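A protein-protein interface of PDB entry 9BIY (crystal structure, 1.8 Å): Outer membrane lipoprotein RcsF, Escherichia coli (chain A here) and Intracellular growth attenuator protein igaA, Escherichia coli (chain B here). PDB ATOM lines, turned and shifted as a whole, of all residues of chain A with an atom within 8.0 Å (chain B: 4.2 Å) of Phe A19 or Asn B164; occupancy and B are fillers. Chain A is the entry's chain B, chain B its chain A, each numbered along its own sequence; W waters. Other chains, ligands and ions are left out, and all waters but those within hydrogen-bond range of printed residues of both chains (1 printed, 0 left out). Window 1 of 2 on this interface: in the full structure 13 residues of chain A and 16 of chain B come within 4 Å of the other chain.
ND2 of Asn B164 sits at hydrogen-bond distance from O of Asp B113 (2.9 Å). The side-chain amide oxygen (OD1) of Asn B164 lies close to the backbone carbonyl oxygen (O) of Gly B162. OG1 of Thr A88 is in hydrogen-bond range of O of Pro A18, 2.8 Å away. The backbone NH (N) of Arg A20 sits at hydrogen-bond distance from the backbone carbonyl oxygen (O) of Asn A86 (2.8 Å). The backbone NH (N) of Ser A83 is in hydrogen-bond range of the backbone carbonyl oxygen (O) of Leu A61 (2.8 Å).
Water W1 lies within hydrogen-bond range of OD1 of Asn B164, O of Gly B162 and N of Asp A21.
Of chain B, only Leu B111, Val B163 and Asn B164 come within 4 Å of Phe A19. Printed residues of chain B within 4 Å of Asp A21: Val B96 (3.9 Å), Leu B100 (3.5 Å) and Asn B164 (3.7 Å). Printed residues of chain B within 4 Å of Ser A83: Leu B100 (3.3 Å). Ala A84 touches none of the printed residues of chain B. Of the printed residues of chain A, Leu B100 touches Asp A21, Leu A61 and Ser A83. Of the printed residues of chain A, Leu B111 touches Phe A19. Of the printed residues of chain A, Val B163 touches Pro A18, Phe A19 and Arg A20. Asn B164 touches just these residues of chain A: Pro A18 (3.4 Å), Phe A19 (2.8 Å), Arg A20 (3.98 Å) and Asp A21 (3.7 Å). The nearest residue of chain B that does not touch Phe A19 is Leu B100 (4.1 Å). The nearest printed residue of chain B that does not touch Ser A83 is Val B96 (7.4 Å).
CB of Pro A18 touches CG1 of Val B163 (3.6 Å). O of Asn B164 touches CA of Pro A18, 3.4 Å away. Phe A19 touches Leu B111 (CZ to CD1, 3.9 Å). Val B163 touches Phe A19. CA of Arg A20 touches OD1 of Asn B164, 3.98 Å away. OD2 of Asp A21 touches CB of Val B96, 3.9 Å away. Asp A21 touches Leu B100 (OD2 to CD2, 3.5 Å). Asn B164 touches Asp A21 (OD1 to N, 3.7 Å). Leu B100 touches Leu A61. Ser A83 touches Leu B100.
O of Phe A19 lies within hydrogen-bond range of N of Asn B164, 2.8 Å away.
Of the 19 printed residues of chain A, 6 touch a printed residue of chain B. Among the printed residues, no Asp or Glu carboxylate lies within 4 Å of a Lys or Arg side-chain nitrogen of the other chain.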
ATOM      1  N   ALA A  11      20.351  25.689  -7.084  1.00  0.00           N
ATOM      2  CA  ALA A  11      21.794  25.544  -6.953  1.00  0.00           C
ATOM      3  C   ALA A  11      22.173  25.063  -5.561  1.00  0.00           C
ATOM      4  O   ALA A  11      23.124  24.287  -5.409  1.00  0.00           O
ATOM      5  CB  ALA A  11      22.481  26.872  -7.264  1.00  0.00           C
ATOM      6  N   LEU A  14      23.360  21.457  -4.932  1.00  0.00           N
ATOM      7  CA  LEU A  14      24.649  20.953  -5.383  1.00  0.00           C
ATOM      8  C   LEU A  14      25.811  21.411  -4.510  1.00  0.00           C
ATOM      9  O   LEU A  14      26.952  21.023  -4.776  1.00  0.00           O
ATOM     10  CB  LEU A  14      24.903  21.386  -6.827  1.00  0.00           C
ATOM     11  CG  LEU A  14      24.054  20.665  -7.874  1.00  0.00           C
ATOM     12  CD1 LEU A  14      23.837  21.595  -9.042  1.00  0.00           C
ATOM     13  CD2 LEU A  14      24.699  19.360  -8.321  1.00  0.00           C
ATOM     14  N   VAL A  15      25.551  22.228  -3.487  1.00  0.00           N
ATOM     15  CA  VAL A  15      26.615  22.688  -2.601  1.00  0.00           C
ATOM     16  C   VAL A  15      27.357  21.494  -2.016  1.00  0.00           C
ATOM     17  O   VAL A  15      26.750  20.577  -1.450  1.00  0.00           O
ATOM     18  CB  VAL A  15      26.036  23.594  -1.505  1.00  0.00           C
ATOM     19  CG1 VAL A  15      26.883  23.526  -0.246  1.00  0.00           C
ATOM     20  CG2 VAL A  15      25.949  25.033  -2.005  1.00  0.00           C
ATOM     21  N   GLY A  16      28.682  21.496  -2.165  1.00  0.00           N
ATOM     22  CA  GLY A  16      29.475  20.378  -1.700  1.00  0.00           C
ATOM     23  C   GLY A  16      29.404  19.166  -2.595  1.00  0.00           C
ATOM     24  O   GLY A  16      29.449  18.032  -2.103  1.00  0.00           O
ATOM     25  N   LYS A  17      29.257  19.378  -3.899  1.00  0.00           N
ATOM     26  CA  LYS A  17      29.285  18.304  -4.889  1.00  0.00           C
ATOM     27  C   LYS A  17      30.126  18.827  -6.041  1.00  0.00           C
ATOM     28  O   LYS A  17      29.627  19.593  -6.882  1.00  0.00           O
ATOM     29  CB  LYS A  17      27.888  17.919  -5.368  1.00  0.00           C
ATOM     30  CG  LYS A  17      26.983  17.346  -4.298  1.00  0.00           C
ATOM     31  CD  LYS A  17      25.626  16.969  -4.887  1.00  0.00           C
ATOM     32  CE  LYS A  17      24.951  15.889  -4.078  1.00  0.00           C
ATOM     33  NZ  LYS A  17      25.019  14.574  -4.773  1.00  0.00           N
ATOM     34  N   PRO A  18      31.408  18.478  -6.092  1.00  0.00           N
ATOM     35  CA  PRO A  18      32.200  18.810  -7.275  1.00  0.00           C
ATOM     36  C   PRO A  18      31.520  18.255  -8.516  1.00  0.00           C
ATOM     37  O   PRO A  18      30.979  17.145  -8.509  1.00  0.00           O
ATOM     38  CB  PRO A  18      33.553  18.141  -7.001  1.00  0.00           C
ATOM     39  CG  PRO A  18      33.603  17.987  -5.501  1.00  0.00           C
ATOM     40  CD  PRO A  18      32.191  17.764  -5.067  1.00  0.00           C
ATOM     41  N   PHE A  19      31.496  19.073  -9.564  1.00  0.00           N
ATOM     42  CA  PHE A  19      30.823  18.732 -10.806  1.00  0.00           C
ATOM     43  C   PHE A  19      31.556  19.420 -11.940  1.00  0.00           C
ATOM     44  O   PHE A  19      32.241  20.428 -11.743  1.00  0.00           O
ATOM     45  CB  PHE A  19      29.340  19.146 -10.793  1.00  0.00           C
ATOM     46  CG  PHE A  19      29.110  20.632 -10.848  1.00  0.00           C
ATOM     47  CD1 PHE A  19      29.042  21.303 -12.065  1.00  0.00           C
ATOM     48  CD2 PHE A  19      28.952  21.363  -9.682  1.00  0.00           C
ATOM     49  CE1 PHE A  19      28.847  22.678 -12.113  1.00  0.00           C
ATOM     50  CE2 PHE A  19      28.754  22.734  -9.718  1.00  0.00           C
ATOM     51  CZ  PHE A  19      28.693  23.394 -10.937  1.00  0.00           C
ATOM     52  N   ARG A  20      31.400  18.865 -13.133  1.00  0.00           N
ATOM     53  CA  ARG A  20      31.837  19.502 -14.363  1.00  0.00           C
ATOM     54  C   ARG A  20      30.613  19.997 -15.120  1.00  0.00           C
ATOM     55  O   ARG A  20      29.571  19.341 -15.123  1.00  0.00           O
ATOM     56  CB  ARG A  20      32.632  18.529 -15.234  1.00  0.00           C
ATOM     57  CG  ARG A  20      33.470  17.542 -14.455  1.00  0.00           C
ATOM     58  CD  ARG A  20      34.928  17.672 -14.841  1.00  0.00           C
ATOM     59  NE  ARG A  20      35.694  16.492 -14.458  1.00  0.00           N
ATOM     60  CZ  ARG A  20      37.013  16.483 -14.294  1.00  0.00           C
ATOM     61  NH1 ARG A  20      37.716  17.595 -14.482  1.00  0.00           N
ATOM     62  NH2 ARG A  20      37.625  15.360 -13.932  1.00  0.00           N
ATOM     63  N   ASP A  21      30.741  21.161 -15.747  1.00  0.00           N
ATOM     64  CA  ASP A  21      29.666  21.733 -16.540  1.00  0.00           C
ATOM     65  C   ASP A  21      29.792  21.267 -17.985  1.00  0.00           C
ATOM     66  O   ASP A  21      30.893  21.198 -18.536  1.00  0.00           O
ATOM     67  CB  ASP A  21      29.700  23.261 -16.458  1.00  0.00           C
ATOM     68  CG  ASP A  21      28.627  23.922 -17.309  1.00  0.00           C
ATOM     69  OD1 ASP A  21      27.576  23.294 -17.556  1.00  0.00           O
ATOM     70  OD2 ASP A  21      28.837  25.079 -17.730  1.00  0.00           O
ATOM     71  N   LEU A  22      28.658  20.925 -18.595  1.00  0.00           N
ATOM     72  CA  LEU A  22      28.665  20.407 -19.959  1.00  0.00           C
ATOM     73  C   LEU A  22      27.810  21.235 -20.904  1.00  0.00           C
ATOM     74  O   LEU A  22      27.585  20.813 -22.044  1.00  0.00           O
ATOM     75  CB  LEU A  22      28.208  18.947 -19.984  1.00  0.00           C
ATOM     76  CG  LEU A  22      28.987  17.935 -19.143  1.00  0.00           C
ATOM     77  CD1 LEU A  22      28.468  17.939 -17.743  1.00  0.00           C
ATOM     78  CD2 LEU A  22      28.853  16.538 -19.718  1.00  0.00           C
ATOM     79  N   ASN A  58      24.907  13.654 -15.905  1.00  0.00           N
ATOM     80  CA  ASN A  58      24.778  12.967 -14.635  1.00  0.00           C
ATOM     81  C   ASN A  58      23.580  13.584 -13.933  1.00  0.00           C
ATOM     82  O   ASN A  58      22.940  12.961 -13.084  1.00  0.00           O
ATOM     83  CB  ASN A  58      26.088  13.156 -13.838  1.00  0.00           C
ATOM     84  CG  ASN A  58      26.030  12.615 -12.424  1.00  0.00           C
ATOM     85  OD1 ASN A  58      25.152  12.961 -11.636  1.00  0.00           O
ATOM     86  ND2 ASN A  58      27.004  11.785 -12.082  1.00  0.00           N
ATOM     87  N   ALA A  59      23.305  14.837 -14.273  1.00  0.00           N
ATOM     88  CA  ALA A  59      22.316  15.647 -13.580  1.00  0.00           C
ATOM     89  C   ALA A  59      22.087  16.916 -14.386  1.00  0.00           C
ATOM     90  O   ALA A  59      22.815  17.219 -15.334  1.00  0.00           O
ATOM     91  CB  ALA A  59      22.752  15.992 -12.154  1.00  0.00           C
ATOM     92  N   LEU A  61      20.904  21.123 -13.622  1.00  0.00           N
ATOM     93  CA  LEU A  61      20.454  22.253 -12.826  1.00  0.00           C
ATOM     94  C   LEU A  61      19.463  23.041 -13.672  1.00  0.00           C
ATOM     95  O   LEU A  61      19.833  23.594 -14.709  1.00  0.00           O
ATOM     96  CB  LEU A  61      21.632  23.136 -12.403  1.00  0.00           C
ATOM     97  CG  LEU A  61      21.235  24.457 -11.741  1.00  0.00           C
ATOM     98  CD1 LEU A  61      20.419  24.201 -10.477  1.00  0.00           C
ATOM     99  CD2 LEU A  61      22.461  25.328 -11.442  1.00  0.00           C
ATOM    100  N   SER A  83      21.322  23.562 -17.129  1.00  0.00           N
ATOM    101  CA  SER A  83      22.710  23.182 -17.367  1.00  0.00           C
ATOM    102  C   SER A  83      22.881  21.680 -17.177  1.00  0.00           C
ATOM    103  O   SER A  83      22.479  21.133 -16.142  1.00  0.00           O
ATOM    104  CB  SER A  83      23.665  23.930 -16.423  1.00  0.00           C
ATOM    105  OG  SER A  83      24.181  25.095 -17.033  1.00  0.00           O
ATOM    106  N   ALA A  84      23.484  21.020 -18.163  1.00  0.00           N
ATOM    107  CA  ALA A  84      23.871  19.626 -17.990  1.00  0.00           C
ATOM    108  C   ALA A  84      25.112  19.555 -17.111  1.00  0.00           C
ATOM    109  O   ALA A  84      26.086  20.278 -17.343  1.00  0.00           O
ATOM    110  CB  ALA A  84      24.145  18.971 -19.338  1.00  0.00           C
ATOM    111  N   LEU A  85      25.082  18.683 -16.102  1.00  0.00           N
ATOM    112  CA  LEU A  85      26.167  18.572 -15.137  1.00  0.00           C
ATOM    113  C   LEU A  85      26.651  17.136 -15.047  1.00  0.00           C
ATOM    114  O   LEU A  85      25.879  16.186 -15.215  1.00  0.00           O
ATOM    115  CB  LEU A  85      25.737  19.032 -13.752  1.00  0.00           C
ATOM    116  CG  LEU A  85      25.177  20.444 -13.685  1.00  0.00           C
ATOM    117  CD1 LEU A  85      24.919  20.809 -12.246  1.00  0.00           C
ATOM    118  CD2 LEU A  85      26.128  21.434 -14.335  1.00  0.00           C
ATOM    119  N   ASN A  86      27.943  16.990 -14.769  1.00  0.00           N
ATOM    120  CA  ASN A  86      28.554  15.695 -14.488  1.00  0.00           C
ATOM    121  C   ASN A  86      29.068  15.769 -13.057  1.00  0.00           C
ATOM    122  O   ASN A  86      30.108  16.383 -12.802  1.00  0.00           O
ATOM    123  CB  ASN A  86      29.675  15.371 -15.472  1.00  0.00           C
ATOM    124  CG  ASN A  86      30.559  14.227 -14.995  1.00  0.00           C
ATOM    125  OD1 ASN A  86      30.104  13.320 -14.294  1.00  0.00           O
ATOM    126  ND2 ASN A  86      31.835  14.273 -15.365  1.00  0.00           N
ATOM    127  N   ILE A  87      28.321  15.173 -12.128  1.00  0.00           N
ATOM    128  CA  ILE A  87      28.765  15.100 -10.743  1.00  0.00           C
ATOM    129  C   ILE A  87      29.873  14.062 -10.640  1.00  0.00           C
ATOM    130  O   ILE A  87      29.724  12.928 -11.119  1.00  0.00           O
ATOM    131  CB  ILE A  87      27.595  14.754  -9.809  1.00  0.00           C
ATOM    132  CG1 ILE A  87      26.338  15.544 -10.179  1.00  0.00           C
ATOM    133  CG2 ILE A  87      27.979  15.009  -8.361  1.00  0.00           C
ATOM    134  CD1 ILE A  87      26.540  17.022 -10.264  1.00  0.00           C
ATOM    135  N   THR A  88      30.989  14.445 -10.017  1.00  0.00           N
ATOM    136  CA  THR A  88      32.168  13.580  -9.944  1.00  0.00           C
ATOM    137  C   THR A  88      31.939  12.355  -9.065  1.00  0.00           C
ATOM    138  O   THR A  88      31.299  12.445  -8.022  1.00  0.00           O
ATOM    139  CB  THR A  88      33.406  14.350  -9.422  1.00  0.00           C
ATOM    140  OG1 THR A  88      33.028  15.213  -8.345  1.00  0.00           O
ATOM    141  CG2 THR A  88      33.993  15.192 -10.531  1.00  0.00           C
ATOM    142  N   VAL B  96      33.211  28.447 -16.745  1.00  0.00           N
ATOM    143  CA  VAL B  96      31.989  27.691 -16.988  1.00  0.00           C
ATOM    144  C   VAL B  96      31.288  28.297 -18.193  1.00  0.00           C
ATOM    145  O   VAL B  96      31.665  29.357 -18.693  1.00  0.00           O
ATOM    146  CB  VAL B  96      31.039  27.662 -15.775  1.00  0.00           C
ATOM    147  CG1 VAL B  96      31.694  26.964 -14.598  1.00  0.00           C
ATOM    148  CG2 VAL B  96      30.616  29.078 -15.402  1.00  0.00           C
ATOM    149  N   LEU B 100      25.363  28.778 -17.577  1.00  0.00           N
ATOM    150  CA  LEU B 100      25.507  28.459 -16.160  1.00  0.00           C
ATOM    151  C   LEU B 100      26.075  29.640 -15.389  1.00  0.00           C
ATOM    152  O   LEU B 100      25.650  29.909 -14.259  1.00  0.00           O
ATOM    153  CB  LEU B 100      26.397  27.235 -15.974  1.00  0.00           C
ATOM    154  CG  LEU B 100      26.764  26.942 -14.517  1.00  0.00           C
ATOM    155  CD1 LEU B 100      25.519  26.546 -13.711  1.00  0.00           C
ATOM    156  CD2 LEU B 100      27.833  25.870 -14.446  1.00  0.00           C
ATOM    157  N   LEU B 111      30.149  30.398  -6.989  1.00  0.00           N
ATOM    158  CA  LEU B 111      30.735  29.272  -7.699  1.00  0.00           C
ATOM    159  C   LEU B 111      32.253  29.387  -7.715  1.00  0.00           C
ATOM    160  O   LEU B 111      32.800  30.478  -7.905  1.00  0.00           O
ATOM    161  CB  LEU B 111      30.218  29.219  -9.141  1.00  0.00           C
ATOM    162  CG  LEU B 111      30.912  28.265 -10.115  1.00  0.00           C
ATOM    163  CD1 LEU B 111      30.184  26.941 -10.151  1.00  0.00           C
ATOM    164  CD2 LEU B 111      30.979  28.880 -11.502  1.00  0.00           C
ATOM    165  N   LEU B 112      32.931  28.257  -7.525  1.00  0.00           N
ATOM    166  CA  LEU B 112      34.353  28.157  -7.813  1.00  0.00           C
ATOM    167  C   LEU B 112      34.529  27.642  -9.242  1.00  0.00           C
ATOM    168  O   LEU B 112      34.138  26.512  -9.559  1.00  0.00           O
ATOM    169  CB  LEU B 112      35.058  27.253  -6.801  1.00  0.00           C
ATOM    170  CG  LEU B 112      35.282  27.861  -5.410  1.00  0.00           C
ATOM    171  CD1 LEU B 112      36.009  26.888  -4.508  1.00  0.00           C
ATOM    172  CD2 LEU B 112      36.057  29.179  -5.492  1.00  0.00           C
ATOM    173  N   ASP B 113      35.094  28.501 -10.096  1.00  0.00           N
ATOM    174  CA  ASP B 113      35.387  28.195 -11.498  1.00  0.00           C
ATOM    175  C   ASP B 113      36.261  26.969 -11.670  1.00  0.00           C
ATOM    176  O   ASP B 113      36.181  26.290 -12.698  1.00  0.00           O
ATOM    177  CB  ASP B 113      36.143  29.370 -12.126  1.00  0.00           C
ATOM    178  CG  ASP B 113      35.246  30.315 -12.836  1.00  0.00           C
ATOM    179  OD1 ASP B 113      34.016  30.166 -12.693  1.00  0.00           O
ATOM    180  OD2 ASP B 113      35.767  31.202 -13.536  1.00  0.00           O
ATOM    181  N   GLY B 162      39.478  22.177 -13.887  1.00  0.00           N
ATOM    182  CA  GLY B 162      38.203  22.697 -14.339  1.00  0.00           C
ATOM    183  C   GLY B 162      36.978  22.130 -13.651  1.00  0.00           C
ATOM    184  O   GLY B 162      35.857  22.477 -14.045  1.00  0.00           O
ATOM    185  N   VAL B 163      37.147  21.249 -12.660  1.00  0.00           N
ATOM    186  CA  VAL B 163      36.041  20.867 -11.793  1.00  0.00           C
ATOM    187  C   VAL B 163      35.518  22.102 -11.079  1.00  0.00           C
ATOM    188  O   VAL B 163      36.291  22.963 -10.635  1.00  0.00           O
ATOM    189  CB  VAL B 163      36.498  19.801 -10.785  1.00  0.00           C
ATOM    190  CG1 VAL B 163      35.478  19.631  -9.674  1.00  0.00           C
ATOM    191  CG2 VAL B 163      36.748  18.480 -11.482  1.00  0.00           C
ATOM    192  N   ASN B 164      34.194  22.259 -11.024  1.00  0.00           N
ATOM    193  CA  ASN B 164      33.586  23.373 -10.311  1.00  0.00           C
ATOM    194  C   ASN B 164      33.003  22.920  -8.973  1.00  0.00           C
ATOM    195  O   ASN B 164      32.635  21.766  -8.813  1.00  0.00           O
ATOM    196  CB  ASN B 164      32.481  24.021 -11.141  1.00  0.00           C
ATOM    197  CG  ASN B 164      32.856  24.178 -12.594  1.00  0.00           C
ATOM    198  OD1 ASN B 164      32.650  23.275 -13.399  1.00  0.00           O
ATOM    199  ND2 ASN B 164      33.406  25.329 -12.937  1.00  0.00           N
ATOM    200  N   VAL B 165      32.996  23.817  -7.989  1.00  0.00           N
ATOM    201  CA  VAL B 165      32.414  23.565  -6.677  1.00  0.00           C
ATOM    202  C   VAL B 165      31.521  24.744  -6.329  1.00  0.00           C
ATOM    203  O   VAL B 165      31.915  25.904  -6.491  1.00  0.00           O
ATOM    204  CB  VAL B 165      33.485  23.343  -5.588  1.00  0.00           C
ATOM    205  CG1 VAL B 165      32.828  22.984  -4.276  1.00  0.00           C
ATOM    206  CG2 VAL B 165      34.435  22.230  -5.992  1.00  0.00           C
HETATM  207  O   HOH W   1      33.531  22.453 -16.058  1.00  0.00           O
